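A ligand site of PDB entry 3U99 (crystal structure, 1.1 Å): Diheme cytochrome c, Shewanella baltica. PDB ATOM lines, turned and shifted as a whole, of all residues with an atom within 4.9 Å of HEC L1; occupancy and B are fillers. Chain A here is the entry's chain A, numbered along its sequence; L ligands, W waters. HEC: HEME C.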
ATOM      1  N   TYR A  26     -11.508  24.788   8.974  1.00  0.00           N
ATOM      2  CA  TYR A  26     -11.330  26.024   9.720  1.00  0.00           C
ATOM      3  C   TYR A  26     -10.448  27.008   8.964  1.00  0.00           C
ATOM      4  O   TYR A  26      -9.348  26.646   8.552  1.00  0.00           O
ATOM      5  CB  TYR A  26     -10.696  25.764  11.072  1.00  0.00           C
ATOM      6  CG  TYR A  26     -11.565  24.894  11.963  1.00  0.00           C
ATOM      7  CD1 TYR A  26     -12.787  25.379  12.430  1.00  0.00           C
ATOM      8  CD2 TYR A  26     -11.201  23.621  12.320  1.00  0.00           C
ATOM      9  CE1 TYR A  26     -13.584  24.581  13.229  1.00  0.00           C
ATOM     10  CE2 TYR A  26     -11.988  22.821  13.119  1.00  0.00           C
ATOM     11  CZ  TYR A  26     -13.196  23.324  13.578  1.00  0.00           C
ATOM     12  OH  TYR A  26     -13.942  22.466  14.358  1.00  0.00           O
ATOM     13  N   LEU A  30      -7.672  31.738  11.920  1.00  0.00           N
ATOM     14  CA  LEU A  30      -8.228  31.560  13.268  1.00  0.00           C
ATOM     15  C   LEU A  30      -7.192  31.163  14.315  1.00  0.00           C
ATOM     16  O   LEU A  30      -7.504  31.230  15.508  1.00  0.00           O
ATOM     17  CB  LEU A  30      -9.375  30.541  13.301  1.00  0.00           C
ATOM     18  CG  LEU A  30     -10.610  30.987  12.482  1.00  0.00           C
ATOM     19  CD1 LEU A  30     -11.603  29.848  12.442  1.00  0.00           C
ATOM     20  CD2 LEU A  30     -11.251  32.219  13.076  1.00  0.00           C
ATOM     21  N   ILE A  91      -9.251  26.057  18.723  1.00  0.00           N
ATOM     22  CA  ILE A  91      -9.780  27.417  18.497  1.00  0.00           C
ATOM     23  C   ILE A  91     -10.706  27.823  19.636  1.00  0.00           C
ATOM     24  O   ILE A  91     -10.663  28.946  20.087  1.00  0.00           O
ATOM     25  CB  ILE A  91     -10.462  27.493  17.155  1.00  0.00           C
ATOM     26  CG1 ILE A  91      -9.462  27.257  16.017  1.00  0.00           C
ATOM     27  CG2 ILE A  91     -11.096  28.852  16.972  1.00  0.00           C
ATOM     28  CD1 ILE A  91     -10.106  26.906  14.674  1.00  0.00           C
ATOM     29  N   THR A  92     -11.526  26.883  20.056  1.00  0.00           N
ATOM     30  CA  THR A  92     -12.566  27.184  21.073  1.00  0.00           C
ATOM     31  C   THR A  92     -11.941  27.394  22.440  1.00  0.00           C
ATOM     32  O   THR A  92     -12.704  27.726  23.378  1.00  0.00           O
ATOM     33  CB  THR A  92     -13.622  26.065  21.109  1.00  0.00           C
ATOM     34  OG1 THR A  92     -12.942  24.821  21.270  1.00  0.00           O
ATOM     35  CG2 THR A  92     -14.429  26.040  19.815  1.00  0.00           C
ATOM     36  N   PHE A  97     -11.997  33.686  21.245  1.00  0.00           N
ATOM     37  CA  PHE A  97     -13.176  32.912  20.963  1.00  0.00           C
ATOM     38  C   PHE A  97     -14.059  32.957  22.213  1.00  0.00           C
ATOM     39  O   PHE A  97     -15.226  33.172  22.124  1.00  0.00           O
ATOM     40  CB  PHE A  97     -12.820  31.436  20.690  1.00  0.00           C
ATOM     41  CG  PHE A  97     -14.023  30.623  20.485  1.00  0.00           C
ATOM     42  CD1 PHE A  97     -14.594  30.561  19.217  1.00  0.00           C
ATOM     43  CD2 PHE A  97     -14.665  30.017  21.531  1.00  0.00           C
ATOM     44  CE1 PHE A  97     -15.771  29.883  19.038  1.00  0.00           C
ATOM     45  CE2 PHE A  97     -15.868  29.356  21.331  1.00  0.00           C
ATOM     46  CZ  PHE A  97     -16.411  29.287  20.085  1.00  0.00           C
ATOM     47  N   LYS A 100     -15.907  36.169  22.662  1.00  0.00           N
ATOM     48  CA  LYS A 100     -16.958  36.412  21.700  1.00  0.00           C
ATOM     49  C   LYS A 100     -18.183  35.558  22.003  1.00  0.00           C
ATOM     50  O   LYS A 100     -19.277  35.969  21.564  1.00  0.00           O
ATOM     51  CB  LYS A 100     -16.440  36.215  20.247  1.00  0.00           C
ATOM     52  CG  LYS A 100     -15.490  37.360  19.882  1.00  0.00           C
ATOM     53  CD  LYS A 100     -14.757  37.080  18.633  1.00  0.00           C
ATOM     54  CE  LYS A 100     -13.781  38.182  18.209  1.00  0.00           C
ATOM     55  NZ  LYS A 100     -14.418  39.528  18.316  1.00  0.00           N
ATOM     56  N   HIS A 101     -18.040  34.467  22.701  1.00  0.00           N
ATOM     57  CA  HIS A 101     -19.171  33.529  22.878  1.00  0.00           C
ATOM     58  C   HIS A 101     -19.671  33.458  24.323  1.00  0.00           C
ATOM     59  O   HIS A 101     -20.525  32.622  24.644  1.00  0.00           O
ATOM     60  CB  HIS A 101     -18.721  32.146  22.395  1.00  0.00           C
ATOM     61  CG  HIS A 101     -18.526  32.167  20.915  1.00  0.00           C
ATOM     62  ND1 HIS A 101     -17.376  32.609  20.342  1.00  0.00           N
ATOM     63  CD2 HIS A 101     -19.351  31.880  19.861  1.00  0.00           C
ATOM     64  CE1 HIS A 101     -17.487  32.581  19.018  1.00  0.00           C
ATOM     65  NE2 HIS A 101     -18.698  32.133  18.674  1.00  0.00           N
ATOM     66  N   GLU A 103     -21.688  35.136  26.195  1.00  0.00           N
ATOM     67  CA  GLU A 103     -23.076  35.424  26.563  1.00  0.00           C
ATOM     68  C   GLU A 103     -24.007  34.336  26.058  1.00  0.00           C
ATOM     69  O   GLU A 103     -25.231  34.416  26.261  1.00  0.00           O
ATOM     70  CB  GLU A 103     -23.448  36.799  26.019  1.00  0.00           C
ATOM     71  CG  GLU A 103     -22.668  37.975  26.596  1.00  0.00           C
ATOM     72  CD  GLU A 103     -22.952  38.218  28.048  1.00  0.00           C
ATOM     73  OE1 GLU A 103     -23.902  37.681  28.713  1.00  0.00           O
ATOM     74  OE2 GLU A 103     -22.181  39.038  28.623  1.00  0.00           O
ATOM     75  N   ILE A 104     -23.507  33.299  25.399  1.00  0.00           N
ATOM     76  CA  ILE A 104     -24.377  32.275  24.800  1.00  0.00           C
ATOM     77  C   ILE A 104     -24.566  31.172  25.834  1.00  0.00           C
ATOM     78  O   ILE A 104     -23.583  30.559  26.258  1.00  0.00           O
ATOM     79  CB  ILE A 104     -23.759  31.722  23.524  1.00  0.00           C
ATOM     80  CG1 ILE A 104     -23.416  32.834  22.522  1.00  0.00           C
ATOM     81  CG2 ILE A 104     -24.673  30.644  22.950  1.00  0.00           C
ATOM     82  CD1 ILE A 104     -22.567  32.302  21.373  1.00  0.00           C
ATOM     83  N   MET A 108     -28.240  26.475  24.628  1.00  0.00           N
ATOM     84  CA  MET A 108     -28.185  26.615  23.162  1.00  0.00           C
ATOM     85  C   MET A 108     -27.008  25.860  22.552  1.00  0.00           C
ATOM     86  O   MET A 108     -26.915  25.807  21.323  1.00  0.00           O
ATOM     87  CB  MET A 108     -28.028  28.081  22.780  1.00  0.00           C
ATOM     88  CG  MET A 108     -29.256  28.910  23.137  1.00  0.00           C
ATOM     89  SD  MET A 108     -29.086  30.621  22.694  1.00  0.00           S
ATOM     90  CE  MET A 108     -30.330  31.348  23.759  1.00  0.00           C
ATOM     91  N   VAL A 109     -26.144  25.308  23.260  1.00  0.00           N
ATOM     92  CA  VAL A 109     -24.861  24.704  22.894  1.00  0.00           C
ATOM     93  C   VAL A 109     -24.775  23.301  23.507  1.00  0.00           C
ATOM     94  O   VAL A 109     -25.223  22.338  22.871  1.00  0.00           O
ATOM     95  CB  VAL A 109     -23.695  25.641  23.251  1.00  0.00           C
ATOM     96  CG1 VAL A 109     -22.381  25.080  22.708  1.00  0.00           C
ATOM     97  CG2 VAL A 109     -23.976  27.059  22.705  1.00  0.00           C
ATOM     98  N   VAL A 115     -26.511  21.162  18.153  1.00  0.00           N
ATOM     99  CA  VAL A 115     -25.208  21.837  18.271  1.00  0.00           C
ATOM    100  C   VAL A 115     -24.173  21.011  19.103  1.00  0.00           C
ATOM    101  O   VAL A 115     -23.192  20.526  18.578  1.00  0.00           O
ATOM    102  CB  VAL A 115     -25.414  23.257  18.884  1.00  0.00           C
ATOM    103  CG1 VAL A 115     -24.124  23.959  19.142  1.00  0.00           C
ATOM    104  CG2 VAL A 115     -26.321  24.082  17.971  1.00  0.00           C
ATOM    105  N   SER A 117     -21.551  21.378  20.894  1.00  0.00           N
ATOM    106  CA  SER A 117     -20.360  22.094  21.276  1.00  0.00           C
ATOM    107  C   SER A 117     -20.108  23.154  20.245  1.00  0.00           C
ATOM    108  O   SER A 117     -20.733  23.204  19.197  1.00  0.00           O
ATOM    109  CB  SER A 117     -19.242  21.064  21.335  1.00  0.00           C
ATOM    110  OG  SER A 117     -18.894  20.646  20.083  1.00  0.00           O
ATOM    111  N   PHE A 118     -19.185  24.047  20.593  1.00  0.00           N
ATOM    112  CA  PHE A 118     -18.867  25.119  19.668  1.00  0.00           C
ATOM    113  C   PHE A 118     -17.966  24.740  18.518  1.00  0.00           C
ATOM    114  O   PHE A 118     -17.755  25.536  17.617  1.00  0.00           O
ATOM    115  CB  PHE A 118     -18.146  26.183  20.488  1.00  0.00           C
ATOM    116  CG  PHE A 118     -19.034  27.075  21.314  1.00  0.00           C
ATOM    117  CD1 PHE A 118     -19.942  27.905  20.722  1.00  0.00           C
ATOM    118  CD2 PHE A 118     -18.918  27.090  22.668  1.00  0.00           C
ATOM    119  CE1 PHE A 118     -20.768  28.718  21.450  1.00  0.00           C
ATOM    120  CE2 PHE A 118     -19.749  27.892  23.445  1.00  0.00           C
ATOM    121  CZ  PHE A 118     -20.643  28.731  22.824  1.00  0.00           C
ATOM    122  N   SER A 119     -17.387  23.563  18.543  1.00  0.00           N
ATOM    123  CA  SER A 119     -16.388  23.209  17.532  1.00  0.00           C
ATOM    124  C   SER A 119     -16.909  23.245  16.120  1.00  0.00           C
ATOM    125  O   SER A 119     -16.157  23.638  15.235  1.00  0.00           O
ATOM    126  CB  SER A 119     -15.853  21.803  17.837  1.00  0.00           C
ATOM    127  OG  SER A 119     -15.137  21.738  19.011  1.00  0.00           O
ATOM    128  N   GLN A 120     -18.108  22.782  15.836  1.00  0.00           N
ATOM    129  CA  GLN A 120     -18.512  22.837  14.413  1.00  0.00           C
ATOM    130  C   GLN A 120     -19.167  24.181  14.188  1.00  0.00           C
ATOM    131  O   GLN A 120     -20.372  24.383  14.316  1.00  0.00           O
ATOM    132  CB  GLN A 120     -19.404  21.665  13.999  1.00  0.00           C
ATOM    133  CG  GLN A 120     -19.868  21.714  12.521  1.00  0.00           C
ATOM    134  CD  GLN A 120     -18.872  21.061  11.580  1.00  0.00           C
ATOM    135  OE1 GLN A 120     -17.688  21.198  11.712  1.00  0.00           O
ATOM    136  NE2 GLN A 120     -19.337  20.344  10.570  1.00  0.00           N
ATOM    137  N   CYS A 121     -18.352  25.169  13.839  1.00  0.00           N
ATOM    138  CA  CYS A 121     -18.871  26.521  13.744  1.00  0.00           C
ATOM    139  C   CYS A 121     -20.004  26.650  12.731  1.00  0.00           C
ATOM    140  O   CYS A 121     -20.830  27.539  12.930  1.00  0.00           O
ATOM    141  CB  CYS A 121     -17.760  27.457  13.244  1.00  0.00           C
ATOM    142  SG  CYS A 121     -16.063  27.154  13.851  1.00  0.00           S
ATOM    143  N   CYS A 124     -23.900  27.129  13.282  1.00  0.00           N
ATOM    144  CA  CYS A 124     -24.453  28.416  13.644  1.00  0.00           C
ATOM    145  C   CYS A 124     -24.094  29.514  12.643  1.00  0.00           C
ATOM    146  O   CYS A 124     -24.864  30.424  12.375  1.00  0.00           O
ATOM    147  CB  CYS A 124     -23.981  28.839  15.027  1.00  0.00           C
ATOM    148  SG  CYS A 124     -24.415  27.679  16.342  1.00  0.00           S
ATOM    149  N   HIS A 125     -22.865  29.458  12.140  1.00  0.00           N
ATOM    150  CA  HIS A 125     -22.317  30.385  11.177  1.00  0.00           C
ATOM    151  C   HIS A 125     -22.286  29.644   9.871  1.00  0.00           C
ATOM    152  O   HIS A 125     -21.325  28.928   9.548  1.00  0.00           O
ATOM    153  CB  HIS A 125     -20.927  30.825  11.585  1.00  0.00           C
ATOM    154  CG  HIS A 125     -20.730  31.480  12.894  1.00  0.00           C
ATOM    155  ND1 HIS A 125     -20.964  32.824  13.081  1.00  0.00           N
ATOM    156  CD2 HIS A 125     -20.247  31.023  14.069  1.00  0.00           C
ATOM    157  CE1 HIS A 125     -20.628  33.128  14.320  1.00  0.00           C
ATOM    158  NE2 HIS A 125     -20.179  32.069  14.971  1.00  0.00           N
ATOM    159  N   PHE A 133     -18.309  35.041   9.878  1.00  0.00           N
ATOM    160  CA  PHE A 133     -18.803  34.769  11.237  1.00  0.00           C
ATOM    161  C   PHE A 133     -19.684  35.856  11.779  1.00  0.00           C
ATOM    162  O   PHE A 133     -20.034  35.829  12.956  1.00  0.00           O
ATOM    163  CB  PHE A 133     -17.595  34.536  12.192  1.00  0.00           C
ATOM    164  CG  PHE A 133     -16.746  33.345  11.814  1.00  0.00           C
ATOM    165  CD1 PHE A 133     -17.111  32.071  12.218  1.00  0.00           C
ATOM    166  CD2 PHE A 133     -15.602  33.449  11.070  1.00  0.00           C
ATOM    167  CE1 PHE A 133     -16.348  30.967  11.867  1.00  0.00           C
ATOM    168  CE2 PHE A 133     -14.861  32.339  10.717  1.00  0.00           C
ATOM    169  CZ  PHE A 133     -15.210  31.084  11.102  1.00  0.00           C
ATOM    170  N   ASP A 134     -20.077  36.788  10.988  1.00  0.00           N
ATOM    171  CA  ASP A 134     -20.801  37.970  11.454  1.00  0.00           C
ATOM    172  C   ASP A 134     -22.029  37.633  12.296  1.00  0.00           C
ATOM    173  O   ASP A 134     -22.865  36.815  11.937  1.00  0.00           O
ATOM    174  CB  ASP A 134     -21.219  38.793  10.256  1.00  0.00           C
ATOM    175  CG  ASP A 134     -20.008  39.315   9.460  1.00  0.00           C
ATOM    176  OD1 ASP A 134     -19.746  40.542   9.388  1.00  0.00           O
ATOM    177  OD2 ASP A 134     -19.328  38.466   8.820  1.00  0.00           O
ATOM    178  N   GLU A 135     -22.135  38.304  13.433  1.00  0.00           N
ATOM    179  CA  GLU A 135     -23.236  38.121  14.369  1.00  0.00           C
ATOM    180  C   GLU A 135     -24.580  38.285  13.714  1.00  0.00           C
ATOM    181  O   GLU A 135     -25.540  37.600  14.092  1.00  0.00           O
ATOM    182  CB  GLU A 135     -23.145  39.035  15.599  1.00  0.00           C
ATOM    183  CG  GLU A 135     -22.899  40.467  15.152  1.00  0.00           C
ATOM    184  CD  GLU A 135     -23.908  41.426  15.701  1.00  0.00           C
ATOM    185  OE1 GLU A 135     -23.661  41.595  16.939  1.00  0.00           O
ATOM    186  OE2 GLU A 135     -24.777  41.949  14.972  1.00  0.00           O
ATOM    187  N   ASP A 136     -24.693  39.170  12.721  1.00  0.00           N
ATOM    188  CA  ASP A 136     -26.004  39.477  12.152  1.00  0.00           C
ATOM    189  C   ASP A 136     -26.475  38.357  11.249  1.00  0.00           C
ATOM    190  O   ASP A 136     -27.626  38.433  10.805  1.00  0.00           O
ATOM    191  CB  ASP A 136     -25.959  40.829  11.427  1.00  0.00           C
ATOM    192  CG  ASP A 136     -24.885  40.992  10.378  1.00  0.00           C
ATOM    193  OD1 ASP A 136     -23.708  41.180  10.772  1.00  0.00           O
ATOM    194  OD2 ASP A 136     -25.210  40.950   9.169  1.00  0.00           O
ATOM    195  N   VAL A 138     -25.726  34.911  12.165  1.00  0.00           N
ATOM    196  CA  VAL A 138     -25.748  33.704  12.977  1.00  0.00           C
ATOM    197  C   VAL A 138     -27.179  33.203  13.156  1.00  0.00           C
ATOM    198  O   VAL A 138     -28.069  33.990  13.387  1.00  0.00           O
ATOM    199  CB  VAL A 138     -25.250  33.975  14.438  1.00  0.00           C
ATOM    200  CG1 VAL A 138     -25.543  32.844  15.423  1.00  0.00           C
ATOM    201  CG2 VAL A 138     -23.787  34.192  14.312  1.00  0.00           C
ATOM    202  N   ILE A 140     -28.800  29.845  15.205  1.00  0.00           N
ATOM    203  CA  ILE A 140     -28.535  28.711  16.081  1.00  0.00           C
ATOM    204  C   ILE A 140     -29.623  27.659  15.897  1.00  0.00           C
ATOM    205  O   ILE A 140     -30.787  27.941  16.111  1.00  0.00           O
ATOM    206  CB  ILE A 140     -28.463  29.149  17.535  1.00  0.00           C
ATOM    207  CG1 ILE A 140     -27.358  30.177  17.710  1.00  0.00           C
ATOM    208  CG2 ILE A 140     -28.300  27.912  18.410  1.00  0.00           C
ATOM    209  CD1 ILE A 140     -27.069  30.470  19.156  1.00  0.00           C
ATOM    210  N   TRP A 146     -29.837  34.909  15.825  1.00  0.00           N
ATOM    211  CA  TRP A 146     -29.438  35.536  17.088  1.00  0.00           C
ATOM    212  C   TRP A 146     -29.867  36.986  17.154  1.00  0.00           C
ATOM    213  O   TRP A 146     -30.315  37.495  18.191  1.00  0.00           O
ATOM    214  CB  TRP A 146     -27.918  35.386  17.135  1.00  0.00           C
ATOM    215  CG  TRP A 146     -27.265  35.977  18.316  1.00  0.00           C
ATOM    216  CD1 TRP A 146     -26.532  37.138  18.328  1.00  0.00           C
ATOM    217  CD2 TRP A 146     -27.257  35.444  19.644  1.00  0.00           C
ATOM    218  NE1 TRP A 146     -26.045  37.339  19.594  1.00  0.00           N
ATOM    219  CE2 TRP A 146     -26.485  36.337  20.402  1.00  0.00           C
ATOM    220  CE3 TRP A 146     -27.833  34.296  20.216  1.00  0.00           C
ATOM    221  CZ2 TRP A 146     -26.297  36.094  21.743  1.00  0.00           C
ATOM    222  CZ3 TRP A 146     -27.606  34.096  21.561  1.00  0.00           C
ATOM    223  CH2 TRP A 146     -26.848  35.005  22.278  1.00  0.00           C
HETATM  224 FE   HEC L   1     -19.467  32.074  16.859  1.00  0.00          FE
HETATM  225  CHA HEC L   1     -20.031  35.402  17.257  1.00  0.00           C
HETATM  226  CHB HEC L   1     -16.434  32.731  15.519  1.00  0.00           C
HETATM  227  CHC HEC L   1     -18.823  28.686  16.757  1.00  0.00           C
HETATM  228  CHD HEC L   1     -22.626  31.456  17.900  1.00  0.00           C
HETATM  229  NA  HEC L   1     -18.457  33.743  16.406  1.00  0.00           N
HETATM  230  C1A HEC L   1     -18.818  35.028  16.642  1.00  0.00           C
HETATM  231  C2A HEC L   1     -17.841  35.960  16.152  1.00  0.00           C
HETATM  232  C3A HEC L   1     -16.834  35.212  15.661  1.00  0.00           C
HETATM  233  C4A HEC L   1     -17.200  33.807  15.839  1.00  0.00           C
HETATM  234  CMA HEC L   1     -15.532  35.669  14.999  1.00  0.00           C
HETATM  235  CAA HEC L   1     -17.960  37.453  16.142  1.00  0.00           C
HETATM  236  CBA HEC L   1     -18.942  37.842  15.048  1.00  0.00           C
HETATM  237  CGA HEC L   1     -19.248  39.327  14.913  1.00  0.00           C
HETATM  238  O1A HEC L   1     -18.410  40.116  15.442  1.00  0.00           O
HETATM  239  O2A HEC L   1     -20.127  39.800  14.192  1.00  0.00           O
HETATM  240  NB  HEC L   1     -17.903  30.957  16.246  1.00  0.00           N
HETATM  241  C1B HEC L   1     -16.690  31.425  15.729  1.00  0.00           C
HETATM  242  C2B HEC L   1     -15.894  30.302  15.430  1.00  0.00           C
HETATM  243  C3B HEC L   1     -16.551  29.199  15.818  1.00  0.00           C
HETATM  244  C4B HEC L   1     -17.823  29.592  16.298  1.00  0.00           C
HETATM  245  CMB HEC L   1     -14.499  30.464  14.786  1.00  0.00           C
HETATM  246  CAB HEC L   1     -16.175  27.713  15.667  1.00  0.00           C
HETATM  247  CBB HEC L   1     -14.724  27.390  16.235  1.00  0.00           C
HETATM  248  NC  HEC L   1     -20.508  30.393  17.280  1.00  0.00           N
HETATM  249  C1C HEC L   1     -20.086  29.142  17.150  1.00  0.00           C
HETATM  250  C2C HEC L   1     -21.103  28.188  17.405  1.00  0.00           C
HETATM  251  C3C HEC L   1     -22.207  28.995  17.691  1.00  0.00           C
HETATM  252  C4C HEC L   1     -21.837  30.345  17.592  1.00  0.00           C
HETATM  253  CMC HEC L   1     -21.034  26.702  17.252  1.00  0.00           C
HETATM  254  CAC HEC L   1     -23.626  28.530  17.942  1.00  0.00           C
HETATM  255  CBC HEC L   1     -23.830  27.684  19.204  1.00  0.00           C
HETATM  256  ND  HEC L   1     -21.012  33.197  17.494  1.00  0.00           N
HETATM  257  C1D HEC L   1     -22.226  32.726  17.871  1.00  0.00           C
HETATM  258  C2D HEC L   1     -23.059  33.809  18.306  1.00  0.00           C
HETATM  259  C3D HEC L   1     -22.313  34.951  18.227  1.00  0.00           C
HETATM  260  C4D HEC L   1     -21.023  34.518  17.656  1.00  0.00           C
HETATM  261  CMD HEC L   1     -24.472  33.666  18.819  1.00  0.00           C
HETATM  262  CAD HEC L   1     -22.784  36.343  18.589  1.00  0.00           C
HETATM  263  CBD HEC L   1     -22.627  36.474  20.150  1.00  0.00           C
HETATM  264  CGD HEC L   1     -23.367  37.674  20.746  1.00  0.00           C
HETATM  265  O1D HEC L   1     -23.012  38.695  19.892  1.00  0.00           O
HETATM  266  O2D HEC L   1     -23.305  37.712  22.066  1.00  0.00           O
HETATM  267 FE   HEC L   2      -9.614  18.217  13.155  1.00  0.00          FE
HETATM  268  CHA HEC L   2     -10.855  19.325  16.069  1.00  0.00           C
HETATM  269  CHB HEC L   2      -7.917  21.126  12.732  1.00  0.00           C
HETATM  270  CHC HEC L   2      -8.510  17.118  10.171  1.00  0.00           C
HETATM  271  CHD HEC L   2     -11.160  15.232  13.687  1.00  0.00           C
HETATM  272  NA  HEC L   2      -9.423  19.925  14.208  1.00  0.00           N
HETATM  273  C1A HEC L   2     -10.060  20.210  15.404  1.00  0.00           C
HETATM  274  C2A HEC L   2      -9.740  21.577  15.793  1.00  0.00           C
HETATM  275  C3A HEC L   2      -8.931  22.074  14.835  1.00  0.00           C
HETATM  276  C4A HEC L   2      -8.714  21.005  13.874  1.00  0.00           C
HETATM  277  CMA HEC L   2      -8.306  23.442  14.795  1.00  0.00           C
HETATM  278  CAA HEC L   2     -10.249  22.201  17.029  1.00  0.00           C
HETATM  279  CBA HEC L   2     -11.667  22.724  16.871  1.00  0.00           C
HETATM  280  CGA HEC L   2     -12.071  23.521  18.111  1.00  0.00           C
HETATM  281  O1A HEC L   2     -11.512  24.636  18.299  1.00  0.00           O
HETATM  282  O2A HEC L   2     -12.909  23.078  18.918  1.00  0.00           O
HETATM  283  NB  HEC L   2      -8.415  18.975  11.723  1.00  0.00           N
HETATM  284  C1B HEC L   2      -7.773  20.194  11.750  1.00  0.00           C
HETATM  285  C2B HEC L   2      -6.886  20.256  10.603  1.00  0.00           C
HETATM  286  C3B HEC L   2      -7.035  19.125   9.893  1.00  0.00           C
HETATM  287  C4B HEC L   2      -8.005  18.336  10.569  1.00  0.00           C
HETATM  288  CMB HEC L   2      -5.982  21.457  10.338  1.00  0.00           C
HETATM  289  CAB HEC L   2      -6.320  18.645   8.626  1.00  0.00           C
HETATM  290  CBB HEC L   2      -4.819  18.478   8.902  1.00  0.00           C
HETATM  291  NC  HEC L   2      -9.823  16.522  12.101  1.00  0.00           N
HETATM  292  C1C HEC L   2      -9.350  16.272  10.864  1.00  0.00           C
HETATM  293  C2C HEC L   2      -9.737  14.994  10.363  1.00  0.00           C
HETATM  294  C3C HEC L   2     -10.491  14.474  11.364  1.00  0.00           C
HETATM  295  C4C HEC L   2     -10.506  15.375  12.445  1.00  0.00           C
HETATM  296  CMC HEC L   2      -9.450  14.473   8.953  1.00  0.00           C
HETATM  297  CAC HEC L   2     -11.215  13.150  11.328  1.00  0.00           C
HETATM  298  CBC HEC L   2     -10.373  11.913  11.069  1.00  0.00           C
HETATM  299  ND  HEC L   2     -10.730  17.430  14.622  1.00  0.00           N
HETATM  300  C1D HEC L   2     -11.232  16.160  14.654  1.00  0.00           C
HETATM  301  C2D HEC L   2     -11.978  15.973  15.907  1.00  0.00           C
HETATM  302  C3D HEC L   2     -11.903  17.131  16.583  1.00  0.00           C
HETATM  303  C4D HEC L   2     -11.154  18.032  15.744  1.00  0.00           C
HETATM  304  CMD HEC L   2     -12.569  14.678  16.424  1.00  0.00           C
HETATM  305  CAD HEC L   2     -12.514  17.392  17.930  1.00  0.00           C
HETATM  306  CBD HEC L   2     -13.948  18.007  17.834  1.00  0.00           C
HETATM  307  CGD HEC L   2     -14.544  18.100  19.228  1.00  0.00           C
HETATM  308  O1D HEC L   2     -15.850  18.408  19.051  1.00  0.00           O
HETATM  309  O2D HEC L   2     -13.715  18.567  20.147  1.00  0.00           O
HETATM  310  O   HOH W   1     -20.143  41.307  11.952  1.00  0.00           O
HETATM  311  O   HOH W   2     -20.570  39.450  18.070  1.00  0.00           O
HETATM  312  O   HOH W   3     -20.553  42.532  14.098  1.00  0.00           O
HETATM  313  O   HOH W   4     -21.312  36.191  23.458  1.00  0.00           O
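The side-chain sulfur of Cys 121 is bonded to a carbon (CAB) of HEC L1, at 1.9 Å.
An iron atom (FE) of HEC L1 is bound by a ring nitrogen (NE2) of His 101, at 2.0 Å.
SG of Cys 124 is bonded to CAC of HEC L1, at 2.0 Å.
A ring nitrogen (NE2) of His 125 binds an iron atom (FE) of HEC L1 (2.0 Å).
The backbone NH (N) of Glu 135 is in hydrogen-bond range of an oxygen (O2A) of HEC L1.
The indole nitrogen of Trp 146 sits close to an oxygen (O1D) of HEC L1.
An oxygen (O1A) of HEC L2 is in hydrogen-bond range of the backbone NH of Thr 92 (2.9 Å).
The side-chain hydroxyl (OG1) of Thr 92 lies within hydrogen-bond range of an oxygen (O2A) of HEC L2 (2.9 Å).
The backbone NH (N) of Ile 91 lies within hydrogen-bond range of an oxygen (O1A) of HEC L2, 2.7 Å away.
An oxygen (O2A) of HEC L2 sits at hydrogen-bond distance from the side-chain hydroxyl (OG) of Ser 119 (2.6 Å).
The backbone carbonyl oxygen of Phe 97 sits at hydrogen-bond distance from a ring nitrogen (ND1) of His 101 (2.8 Å).
The backbone carbonyl oxygen (O) of Phe 133 lies close to a ring nitrogen (ND1) of His 125, at 3.1 Å.
O of Val 138 sits at hydrogen-bond distance from N of Trp 146 (3.1 Å).
Leu 30 touches HEC L1 (CD1 to CMB, 3.8 Å).
Ile 91 touches HEC L1 (CG2 to CBB, 3.98 Å).
Thr 92 touches HEC L1 (CG2 to CBB, 3.8 Å).
Phe 97 touches HEC L1.
Lys 100 touches HEC L1 (O to CBD, 3.7 Å).
CD1 of Ile 104 touches C2D of HEC L1, 3.5 Å away.
CG2 of Val 109 touches CBC of HEC L1, 3.6 Å away.
CG1 of Val 115 touches CBC of HEC L1, 3.7 Å away.
Phe 118 touches HEC L1 (O to CAB, 3.3 Å).
O of Gln 120 touches CMC of HEC L1 (3.8 Å).
Phe 133 touches HEC L1.
Asp 134 touches HEC L1.
CG1 of Val 138 touches CMD of HEC L1, 3.7 Å away.
Hydrophobic or aromatic side chains within 4 Å of HEC L1: Leu 30, Ile 91, Phe 97, His 101, Ile 104, Val 109, Val 115, Phe 118, His 125, Phe 133, Val 138 and Trp 146.
Within 4 Å of HEC L1: Leu 30, Ile 91, Thr 92, Phe 97, Lys 100, His 101, Ile 104, Val 109, Val 115, Phe 118, Gln 120, Cys 121, Cys 124, His 125, Phe 133, Asp 134, Glu 135, Val 138 and Trp 146.
The nearest printed residue that does not touch HEC L1 is Ser 117 (4.01 Å).
Water W1 lies within hydrogen-bond range of an oxygen (O2A) of HEC L1 (2.7 Å) and the side-chain carboxylate (OD1) of Asp 134 (2.7 Å).
Water W4 lies within hydrogen-bond range of O of Lys 100 (2.8 Å), O2D of HEC L1 (2.9 Å) and N of Glu 103 (3.0 Å).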
